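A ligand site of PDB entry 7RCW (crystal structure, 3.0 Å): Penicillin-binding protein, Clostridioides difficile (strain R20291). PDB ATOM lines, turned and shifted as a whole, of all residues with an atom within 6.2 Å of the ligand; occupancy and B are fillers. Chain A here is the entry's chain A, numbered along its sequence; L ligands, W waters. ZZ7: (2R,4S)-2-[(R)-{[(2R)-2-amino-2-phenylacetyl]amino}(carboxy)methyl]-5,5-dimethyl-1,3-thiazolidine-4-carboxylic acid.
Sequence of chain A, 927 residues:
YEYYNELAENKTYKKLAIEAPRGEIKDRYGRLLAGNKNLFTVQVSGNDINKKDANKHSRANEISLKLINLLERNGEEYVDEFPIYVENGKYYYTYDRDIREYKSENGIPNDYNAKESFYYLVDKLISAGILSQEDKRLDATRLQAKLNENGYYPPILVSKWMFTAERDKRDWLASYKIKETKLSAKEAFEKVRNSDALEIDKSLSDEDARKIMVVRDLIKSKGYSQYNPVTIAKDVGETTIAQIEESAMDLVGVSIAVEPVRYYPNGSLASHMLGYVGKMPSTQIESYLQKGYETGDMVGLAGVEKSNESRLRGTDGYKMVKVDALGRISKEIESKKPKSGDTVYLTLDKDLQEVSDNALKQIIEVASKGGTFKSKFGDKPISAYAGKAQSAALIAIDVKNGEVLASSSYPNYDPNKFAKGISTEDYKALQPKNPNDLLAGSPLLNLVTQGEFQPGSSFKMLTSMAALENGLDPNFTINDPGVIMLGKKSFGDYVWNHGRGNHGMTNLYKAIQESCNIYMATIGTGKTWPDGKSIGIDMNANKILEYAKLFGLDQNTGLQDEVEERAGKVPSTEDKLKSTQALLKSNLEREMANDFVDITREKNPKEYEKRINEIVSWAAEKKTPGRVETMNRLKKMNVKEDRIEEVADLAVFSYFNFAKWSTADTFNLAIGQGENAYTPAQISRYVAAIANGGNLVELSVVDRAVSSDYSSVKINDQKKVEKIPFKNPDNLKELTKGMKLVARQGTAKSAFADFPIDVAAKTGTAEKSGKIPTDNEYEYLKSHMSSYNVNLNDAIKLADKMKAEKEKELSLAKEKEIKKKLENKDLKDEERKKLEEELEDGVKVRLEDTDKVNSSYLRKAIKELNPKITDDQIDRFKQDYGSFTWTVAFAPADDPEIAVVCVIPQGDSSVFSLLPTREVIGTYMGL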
ATOM      1  N   GLY A 456      -1.680 -29.842  14.951  1.00  0.00           N
ATOM      2  CA  GLY A 456      -0.870 -29.498  16.122  1.00  0.00           C
ATOM      3  C   GLY A 456      -1.721 -28.883  17.198  1.00  0.00           C
ATOM      4  O   GLY A 456      -2.900 -29.166  17.230  1.00  0.00           O
ATOM      5  N   SER A 457      -1.135 -28.028  18.028  1.00  0.00           N
ATOM      6  CA  SER A 457      -1.856 -27.452  19.176  1.00  0.00           C
ATOM      7  C   SER A 457      -2.403 -26.074  18.850  1.00  0.00           C
ATOM      8  O   SER A 457      -2.911 -25.436  19.740  1.00  0.00           O
ATOM      9  CB  SER A 457      -0.942 -27.440  20.351  1.00  0.00           C
ATOM     10  OG  SER A 457      -0.870 -28.686  21.037  1.00  0.00           O
ATOM     11  N   SER A 458      -2.313 -25.677  17.583  1.00  0.00           N
ATOM     12  CA  SER A 458      -2.974 -24.441  17.118  1.00  0.00           C
ATOM     13  C   SER A 458      -4.477 -24.681  17.197  1.00  0.00           C
ATOM     14  O   SER A 458      -5.219 -23.736  17.459  1.00  0.00           O
ATOM     15  CB  SER A 458      -2.573 -24.154  15.732  1.00  0.00           C
ATOM     16  OG  SER A 458      -3.060 -25.163  14.881  1.00  0.00           O
ATOM     17  N   LYS A 460      -5.966 -25.805  19.375  1.00  0.00           N
ATOM     18  CA  LYS A 460      -6.490 -25.763  20.768  1.00  0.00           C
ATOM     19  C   LYS A 460      -7.493 -24.613  20.965  1.00  0.00           C
ATOM     20  O   LYS A 460      -8.364 -24.777  21.832  1.00  0.00           O
ATOM     21  CB  LYS A 460      -5.382 -25.648  21.831  1.00  0.00           C
ATOM     22  CG  LYS A 460      -4.708 -26.967  22.155  1.00  0.00           C
ATOM     23  CD  LYS A 460      -3.829 -26.976  23.371  1.00  0.00           C
ATOM     24  CE  LYS A 460      -3.263 -28.367  23.637  1.00  0.00           C
ATOM     25  NZ  LYS A 460      -1.981 -28.345  24.379  1.00  0.00           N
ATOM     26  N   GLY A 492      -0.841 -37.248  28.431  1.00  0.00           N
ATOM     27  CA  GLY A 492      -0.222 -36.291  29.371  1.00  0.00           C
ATOM     28  C   GLY A 492       0.489 -35.124  28.709  1.00  0.00           C
ATOM     29  O   GLY A 492       0.893 -35.238  27.557  1.00  0.00           O
ATOM     30  N   ASP A 493       0.673 -34.062  29.479  1.00  0.00           N
ATOM     31  CA  ASP A 493       1.375 -32.828  29.054  1.00  0.00           C
ATOM     32  C   ASP A 493       2.809 -33.183  28.704  1.00  0.00           C
ATOM     33  O   ASP A 493       3.298 -34.201  29.210  1.00  0.00           O
ATOM     34  CB  ASP A 493       1.407 -31.803  30.189  1.00  0.00           C
ATOM     35  CG  ASP A 493       0.045 -31.260  30.622  1.00  0.00           C
ATOM     36  OD1 ASP A 493      -0.926 -31.330  29.837  1.00  0.00           O
ATOM     37  OD2 ASP A 493      -0.043 -30.727  31.734  1.00  0.00           O
ATOM     38  N   TYR A 494       3.438 -32.373  27.868  1.00  0.00           N
ATOM     39  CA  TYR A 494       4.830 -32.591  27.420  1.00  0.00           C
ATOM     40  C   TYR A 494       5.749 -32.507  28.623  1.00  0.00           C
ATOM     41  O   TYR A 494       6.726 -33.239  28.709  1.00  0.00           O
ATOM     42  CB  TYR A 494       5.220 -31.508  26.421  1.00  0.00           C
ATOM     43  CG  TYR A 494       6.696 -31.274  26.296  1.00  0.00           C
ATOM     44  CD1 TYR A 494       7.494 -32.123  25.558  1.00  0.00           C
ATOM     45  CD2 TYR A 494       7.298 -30.185  26.901  1.00  0.00           C
ATOM     46  CE1 TYR A 494       8.850 -31.905  25.433  1.00  0.00           C
ATOM     47  CE2 TYR A 494       8.655 -29.959  26.787  1.00  0.00           C
ATOM     48  CZ  TYR A 494       9.433 -30.819  26.049  1.00  0.00           C
ATOM     49  OH  TYR A 494      10.770 -30.612  25.924  1.00  0.00           O
ATOM     50  N   HIS A 498       8.145 -35.714  30.164  1.00  0.00           N
ATOM     51  CA  HIS A 498       9.613 -35.660  30.339  1.00  0.00           C
ATOM     52  C   HIS A 498       9.946 -35.754  31.826  1.00  0.00           C
ATOM     53  O   HIS A 498      10.402 -36.829  32.252  1.00  0.00           O
ATOM     54  CB  HIS A 498      10.206 -34.511  29.550  1.00  0.00           C
ATOM     55  CG  HIS A 498      10.212 -34.844  28.103  1.00  0.00           C
ATOM     56  ND1 HIS A 498       9.062 -34.810  27.351  1.00  0.00           N
ATOM     57  CD2 HIS A 498      11.182 -35.310  27.296  1.00  0.00           C
ATOM     58  CE1 HIS A 498       9.337 -35.202  26.127  1.00  0.00           C
ATOM     59  NE2 HIS A 498      10.628 -35.507  26.066  1.00  0.00           N
ATOM     60  N   GLU A 514       0.408 -22.078  28.296  1.00  0.00           N
ATOM     61  CA  GLU A 514       1.514 -23.061  28.493  1.00  0.00           C
ATOM     62  C   GLU A 514       1.240 -24.333  27.680  1.00  0.00           C
ATOM     63  O   GLU A 514       2.113 -25.233  27.679  1.00  0.00           O
ATOM     64  CB  GLU A 514       1.713 -23.362  29.980  1.00  0.00           C
ATOM     65  CG  GLU A 514       2.140 -22.158  30.797  1.00  0.00           C
ATOM     66  CD  GLU A 514       3.588 -21.713  30.635  1.00  0.00           C
ATOM     67  OE1 GLU A 514       4.380 -22.446  30.024  1.00  0.00           O
ATOM     68  OE2 GLU A 514       3.911 -20.622  31.124  1.00  0.00           O
ATOM     69  N   SER A 515       0.071 -24.410  27.038  1.00  0.00           N
ATOM     70  CA  SER A 515      -0.401 -25.517  26.166  1.00  0.00           C
ATOM     71  C   SER A 515      -0.694 -26.801  26.972  1.00  0.00           C
ATOM     72  O   SER A 515      -0.308 -27.880  26.510  1.00  0.00           O
ATOM     73  CB  SER A 515       0.570 -25.774  25.049  1.00  0.00           C
ATOM     74  OG  SER A 515      -0.048 -26.481  23.984  1.00  0.00           O
ATOM     75  N   ASN A 517      -2.379 -30.029  27.919  1.00  0.00           N
ATOM     76  CA  ASN A 517      -3.170 -30.984  27.115  1.00  0.00           C
ATOM     77  C   ASN A 517      -4.302 -31.538  27.956  1.00  0.00           C
ATOM     78  O   ASN A 517      -5.357 -31.814  27.416  1.00  0.00           O
ATOM     79  CB  ASN A 517      -2.303 -32.144  26.633  1.00  0.00           C
ATOM     80  CG  ASN A 517      -1.360 -31.727  25.542  1.00  0.00           C
ATOM     81  OD1 ASN A 517      -1.636 -30.780  24.819  1.00  0.00           O
ATOM     82  ND2 ASN A 517      -0.244 -32.409  25.418  1.00  0.00           N
ATOM     83  N   ILE A 671      -6.606 -31.677  20.553  1.00  0.00           N
ATOM     84  CA  ILE A 671      -5.267 -31.010  20.648  1.00  0.00           C
ATOM     85  C   ILE A 671      -4.540 -31.155  19.305  1.00  0.00           C
ATOM     86  O   ILE A 671      -3.285 -31.078  19.296  1.00  0.00           O
ATOM     87  CB  ILE A 671      -4.464 -31.569  21.835  1.00  0.00           C
ATOM     88  CG1 ILE A 671      -4.034 -33.013  21.607  1.00  0.00           C
ATOM     89  CG2 ILE A 671      -5.253 -31.424  23.130  1.00  0.00           C
ATOM     90  CD1 ILE A 671      -2.866 -33.439  22.450  1.00  0.00           C
ATOM     91  N   GLN A 673      -4.461 -33.714  16.978  1.00  0.00           N
ATOM     92  CA  GLN A 673      -3.914 -35.055  16.641  1.00  0.00           C
ATOM     93  C   GLN A 673      -5.074 -35.885  16.051  1.00  0.00           C
ATOM     94  O   GLN A 673      -6.105 -35.290  15.718  1.00  0.00           O
ATOM     95  CB  GLN A 673      -3.219 -35.651  17.867  1.00  0.00           C
ATOM     96  CG  GLN A 673      -1.701 -35.510  17.846  1.00  0.00           C
ATOM     97  CD  GLN A 673      -1.150 -34.950  19.131  1.00  0.00           C
ATOM     98  OE1 GLN A 673      -1.138 -35.601  20.179  1.00  0.00           O
ATOM     99  NE2 GLN A 673      -0.674 -33.712  19.054  1.00  0.00           N
ATOM    100  N   THR A 747       4.847 -20.332  26.005  1.00  0.00           N
ATOM    101  CA  THR A 747       5.765 -21.183  25.220  1.00  0.00           C
ATOM    102  C   THR A 747       6.615 -20.361  24.246  1.00  0.00           C
ATOM    103  O   THR A 747       7.737 -20.793  23.911  1.00  0.00           O
ATOM    104  CB  THR A 747       4.948 -22.211  24.448  1.00  0.00           C
ATOM    105  OG1 THR A 747       3.979 -21.565  23.627  1.00  0.00           O
ATOM    106  CG2 THR A 747       4.249 -23.160  25.398  1.00  0.00           C
ATOM    107  N   LYS A 762       0.187 -18.927  19.075  1.00  0.00           N
ATOM    108  CA  LYS A 762       0.071 -20.293  19.638  1.00  0.00           C
ATOM    109  C   LYS A 762       1.104 -21.166  18.922  1.00  0.00           C
ATOM    110  O   LYS A 762       1.220 -21.058  17.694  1.00  0.00           O
ATOM    111  CB  LYS A 762      -1.364 -20.810  19.491  1.00  0.00           C
ATOM    112  CG  LYS A 762      -1.614 -22.195  20.081  1.00  0.00           C
ATOM    113  CD  LYS A 762      -1.696 -22.241  21.580  1.00  0.00           C
ATOM    114  CE  LYS A 762      -1.313 -23.605  22.135  1.00  0.00           C
ATOM    115  NZ  LYS A 762       0.112 -23.664  22.542  1.00  0.00           N
ATOM    116  N   THR A 763       1.871 -21.926  19.684  1.00  0.00           N
ATOM    117  CA  THR A 763       2.908 -22.897  19.221  1.00  0.00           C
ATOM    118  C   THR A 763       2.273 -24.287  19.100  1.00  0.00           C
ATOM    119  O   THR A 763       1.094 -24.439  19.479  1.00  0.00           O
ATOM    120  CB  THR A 763       4.104 -22.925  20.188  1.00  0.00           C
ATOM    121  OG1 THR A 763       3.642 -22.983  21.535  1.00  0.00           O
ATOM    122  CG2 THR A 763       4.985 -21.711  20.023  1.00  0.00           C
ATOM    123  N   GLY A 764       3.022 -25.250  18.577  1.00  0.00           N
ATOM    124  CA  GLY A 764       2.563 -26.649  18.429  1.00  0.00           C
ATOM    125  C   GLY A 764       3.678 -27.569  17.978  1.00  0.00           C
ATOM    126  O   GLY A 764       4.724 -27.068  17.542  1.00  0.00           O
ATOM    127  N   THR A 765       3.462 -28.873  18.130  1.00  0.00           N
ATOM    128  CA  THR A 765       4.313 -29.970  17.597  1.00  0.00           C
ATOM    129  C   THR A 765       3.432 -31.219  17.564  1.00  0.00           C
ATOM    130  O   THR A 765       2.894 -31.569  18.625  1.00  0.00           O
ATOM    131  CB  THR A 765       5.580 -30.191  18.426  1.00  0.00           C
ATOM    132  OG1 THR A 765       6.260 -28.954  18.639  1.00  0.00           O
ATOM    133  CG2 THR A 765       6.567 -31.110  17.760  1.00  0.00           C
ATOM    134  N   ALA A 766       3.248 -31.825  16.395  1.00  0.00           N
ATOM    135  CA  ALA A 766       2.360 -32.990  16.212  1.00  0.00           C
ATOM    136  C   ALA A 766       3.194 -34.210  15.831  1.00  0.00           C
ATOM    137  O   ALA A 766       3.881 -34.163  14.780  1.00  0.00           O
ATOM    138  CB  ALA A 766       1.340 -32.674  15.146  1.00  0.00           C
ATOM    139  N   GLU A 767       3.120 -35.249  16.659  1.00  0.00           N
ATOM    140  CA  GLU A 767       3.716 -36.588  16.386  1.00  0.00           C
ATOM    141  C   GLU A 767       2.677 -37.427  15.634  1.00  0.00           C
ATOM    142  O   GLU A 767       1.638 -37.808  16.271  1.00  0.00           O
ATOM    143  CB  GLU A 767       4.159 -37.265  17.687  1.00  0.00           C
ATOM    144  CG  GLU A 767       5.234 -38.326  17.504  1.00  0.00           C
ATOM    145  CD  GLU A 767       6.621 -37.765  17.207  1.00  0.00           C
ATOM    146  OE1 GLU A 767       7.123 -36.988  18.051  1.00  0.00           O
ATOM    147  OE2 GLU A 767       7.187 -38.081  16.131  1.00  0.00           O
ATOM    148  N   SER A 883       7.391 -35.980  13.309  1.00  0.00           N
ATOM    149  CA  SER A 883       6.820 -34.779  13.962  1.00  0.00           C
ATOM    150  C   SER A 883       6.829 -33.617  12.971  1.00  0.00           C
ATOM    151  O   SER A 883       7.672 -33.653  12.044  1.00  0.00           O
ATOM    152  CB  SER A 883       7.597 -34.431  15.209  1.00  0.00           C
ATOM    153  OG  SER A 883       8.838 -33.805  14.875  1.00  0.00           O
ATOM    154  N   THR A 885       6.655 -29.285  13.629  1.00  0.00           N
ATOM    155  CA  THR A 885       6.613 -28.164  14.610  1.00  0.00           C
ATOM    156  C   THR A 885       6.019 -26.909  13.951  1.00  0.00           C
ATOM    157  O   THR A 885       6.435 -26.579  12.824  1.00  0.00           O
ATOM    158  CB  THR A 885       7.990 -27.957  15.249  1.00  0.00           C
ATOM    159  OG1 THR A 885       7.873 -26.985  16.290  1.00  0.00           O
ATOM    160  CG2 THR A 885       9.030 -27.439  14.290  1.00  0.00           C
ATOM    161  N   TRP A 886       5.058 -26.259  14.625  1.00  0.00           N
ATOM    162  CA  TRP A 886       4.185 -25.157  14.099  1.00  0.00           C
ATOM    163  C   TRP A 886       4.362 -23.868  14.922  1.00  0.00           C
ATOM    164  O   TRP A 886       4.905 -23.919  16.063  1.00  0.00           O
ATOM    165  CB  TRP A 886       2.698 -25.532  14.139  1.00  0.00           C
ATOM    166  CG  TRP A 886       2.179 -26.510  13.141  1.00  0.00           C
ATOM    167  CD1 TRP A 886       2.156 -27.862  13.273  1.00  0.00           C
ATOM    168  CD2 TRP A 886       1.456 -26.225  11.928  1.00  0.00           C
ATOM    169  NE1 TRP A 886       1.500 -28.440  12.217  1.00  0.00           N
ATOM    170  CE2 TRP A 886       1.072 -27.462  11.370  1.00  0.00           C
ATOM    171  CE3 TRP A 886       1.120 -25.050  11.243  1.00  0.00           C
ATOM    172  CZ2 TRP A 886       0.369 -27.553  10.169  1.00  0.00           C
ATOM    173  CZ3 TRP A 886       0.428 -25.143  10.051  1.00  0.00           C
ATOM    174  CH2 TRP A 886       0.048 -26.378   9.534  1.00  0.00           C
ATOM    175  N   SER A 910      10.609 -25.615  19.254  1.00  0.00           N
ATOM    176  CA  SER A 910       9.487 -24.788  18.727  1.00  0.00           C
ATOM    177  C   SER A 910      10.012 -23.433  18.256  1.00  0.00           C
ATOM    178  O   SER A 910       9.219 -22.640  17.711  1.00  0.00           O
ATOM    179  CB  SER A 910       8.389 -24.604  19.721  1.00  0.00           C
ATOM    180  OG  SER A 910       7.180 -24.305  19.024  1.00  0.00           O
HETATM  181  O1  ZZ7 L   1       3.410 -25.379  21.746  1.00  0.00           O
HETATM  182  C2  ZZ7 L   1       4.214 -26.357  21.706  1.00  0.00           C
HETATM  183  O2  ZZ7 L   1       5.419 -26.340  21.400  1.00  0.00           O
HETATM  184  C12 ZZ7 L   1       3.552 -27.838  22.082  1.00  0.00           C
HETATM  185  C6  ZZ7 L   1       4.211 -28.461  23.337  1.00  0.00           C
HETATM  186  C1  ZZ7 L   1       5.574 -29.070  23.110  1.00  0.00           C
HETATM  187  C16 ZZ7 L   1       4.130 -27.590  24.580  1.00  0.00           C
HETATM  188  S1  ZZ7 L   1       2.994 -29.874  23.677  1.00  0.00           S
HETATM  189  N3  ZZ7 L   1       2.061 -27.797  22.424  1.00  0.00           N
HETATM  190  C13 ZZ7 L   1       1.546 -29.017  22.993  1.00  0.00           C
HETATM  191  C14 ZZ7 L   1       0.850 -30.074  22.090  1.00  0.00           C
HETATM  192  C15 ZZ7 L   1       0.229 -29.411  20.883  1.00  0.00           C
HETATM  193  O4  ZZ7 L   1       0.689 -29.588  19.788  1.00  0.00           O
HETATM  194  N1  ZZ7 L   1       1.692 -31.137  21.493  1.00  0.00           N
HETATM  195  C3  ZZ7 L   1       1.463 -32.455  21.739  1.00  0.00           C
HETATM  196  O3  ZZ7 L   1       0.522 -32.649  22.518  1.00  0.00           O
HETATM  197  C4  ZZ7 L   1       2.223 -33.795  21.093  1.00  0.00           C
HETATM  198  N2  ZZ7 L   1       1.720 -35.056  21.731  1.00  0.00           N
HETATM  199  C5  ZZ7 L   1       3.707 -33.704  21.106  1.00  0.00           C
HETATM  200  C7  ZZ7 L   1       4.477 -34.058  19.953  1.00  0.00           C
HETATM  201  C8  ZZ7 L   1       5.915 -33.941  19.926  1.00  0.00           C
HETATM  202  C9  ZZ7 L   1       6.613 -33.472  21.061  1.00  0.00           C
HETATM  203  C10 ZZ7 L   1       5.859 -33.134  22.216  1.00  0.00           C
HETATM  204  C11 ZZ7 L   1       4.428 -33.239  22.235  1.00  0.00           C
HETATM  205  O   HOH W   1      -0.044 -37.202  23.508  1.00  0.00           O
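The backbone NH of Ser 457 lies close to an oxygen (O4) of the ligand.
A carbon (C15) of the ligand is covalently linked to the side-chain hydroxyl (OG) of Ser 457, 1.3 Å away.
An oxygen (O1) of the ligand lies within hydrogen-bond range of the side-chain hydroxyl (OG1) of Thr 763 (2.4 Å).
The side-chain hydroxyl (OG) of Ser 515 lies within hydrogen-bond range of a nitrogen (N3) of the ligand, 2.9 Å away.
ND2 of Asn 517 is in hydrogen-bond range of O3 of the ligand.
O4 of the ligand is in hydrogen-bond range of N of Thr 765 (3.3 Å).
The backbone carbonyl oxygen (O) of Thr 765 sits at hydrogen-bond distance from a nitrogen (N1) of the ligand (3.1 Å).
O1 of the ligand sits at hydrogen-bond distance from N of Gly 764 (3.2 Å).
OE1 of Gln 673 lies within hydrogen-bond range of N2 of the ligand (3.3 Å).
An oxygen (O1) of the ligand is in salt-bridge range of the side-chain amino group (NZ) of Lys 762, at 3.8 Å.
The side-chain hydroxyl (OG1) of Thr 747 is in hydrogen-bond range of the side-chain hydroxyl (OG1) of Thr 763 (2.5 Å).
The side-chain hydroxyl (OG) of Ser 515 is in hydrogen-bond range of the side-chain amino group (NZ) of Lys 762, at 3.2 Å.
The side-chain hydroxyl (OG) of Ser 515 sits at hydrogen-bond distance from the side-chain amino group (NZ) of Lys 460 (2.7 Å).
The side-chain amide oxygen (OD1) of Asn 517 sits at hydrogen-bond distance from the side-chain amino group (NZ) of Lys 460 (2.5 Å).
The side-chain carboxylate (OD1) of Asp 493 lies within hydrogen-bond range of the backbone NH (N) of Asn 517 (2.7 Å).
OG1 of Thr 765 sits at hydrogen-bond distance from OG1 of Thr 885.
OG1 of Thr 885 sits at hydrogen-bond distance from O of Gly 764.
The backbone carbonyl oxygen of Gly 764 is in hydrogen-bond range of the backbone NH of Trp 886 (3.0 Å).
Residues that only touch the ligand: Ile 671, Ser 910, Gly 456, Glu 767, Lys 460 and Tyr 494.
Hydrophobic or aromatic side chains that line the ligand: Tyr 494 and Ile 671.
Of the 24 residues printed, 14 come within 4 Å of the ligand.
The nearest printed residue that does not touch the ligand is Thr 747 (4.3 Å).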
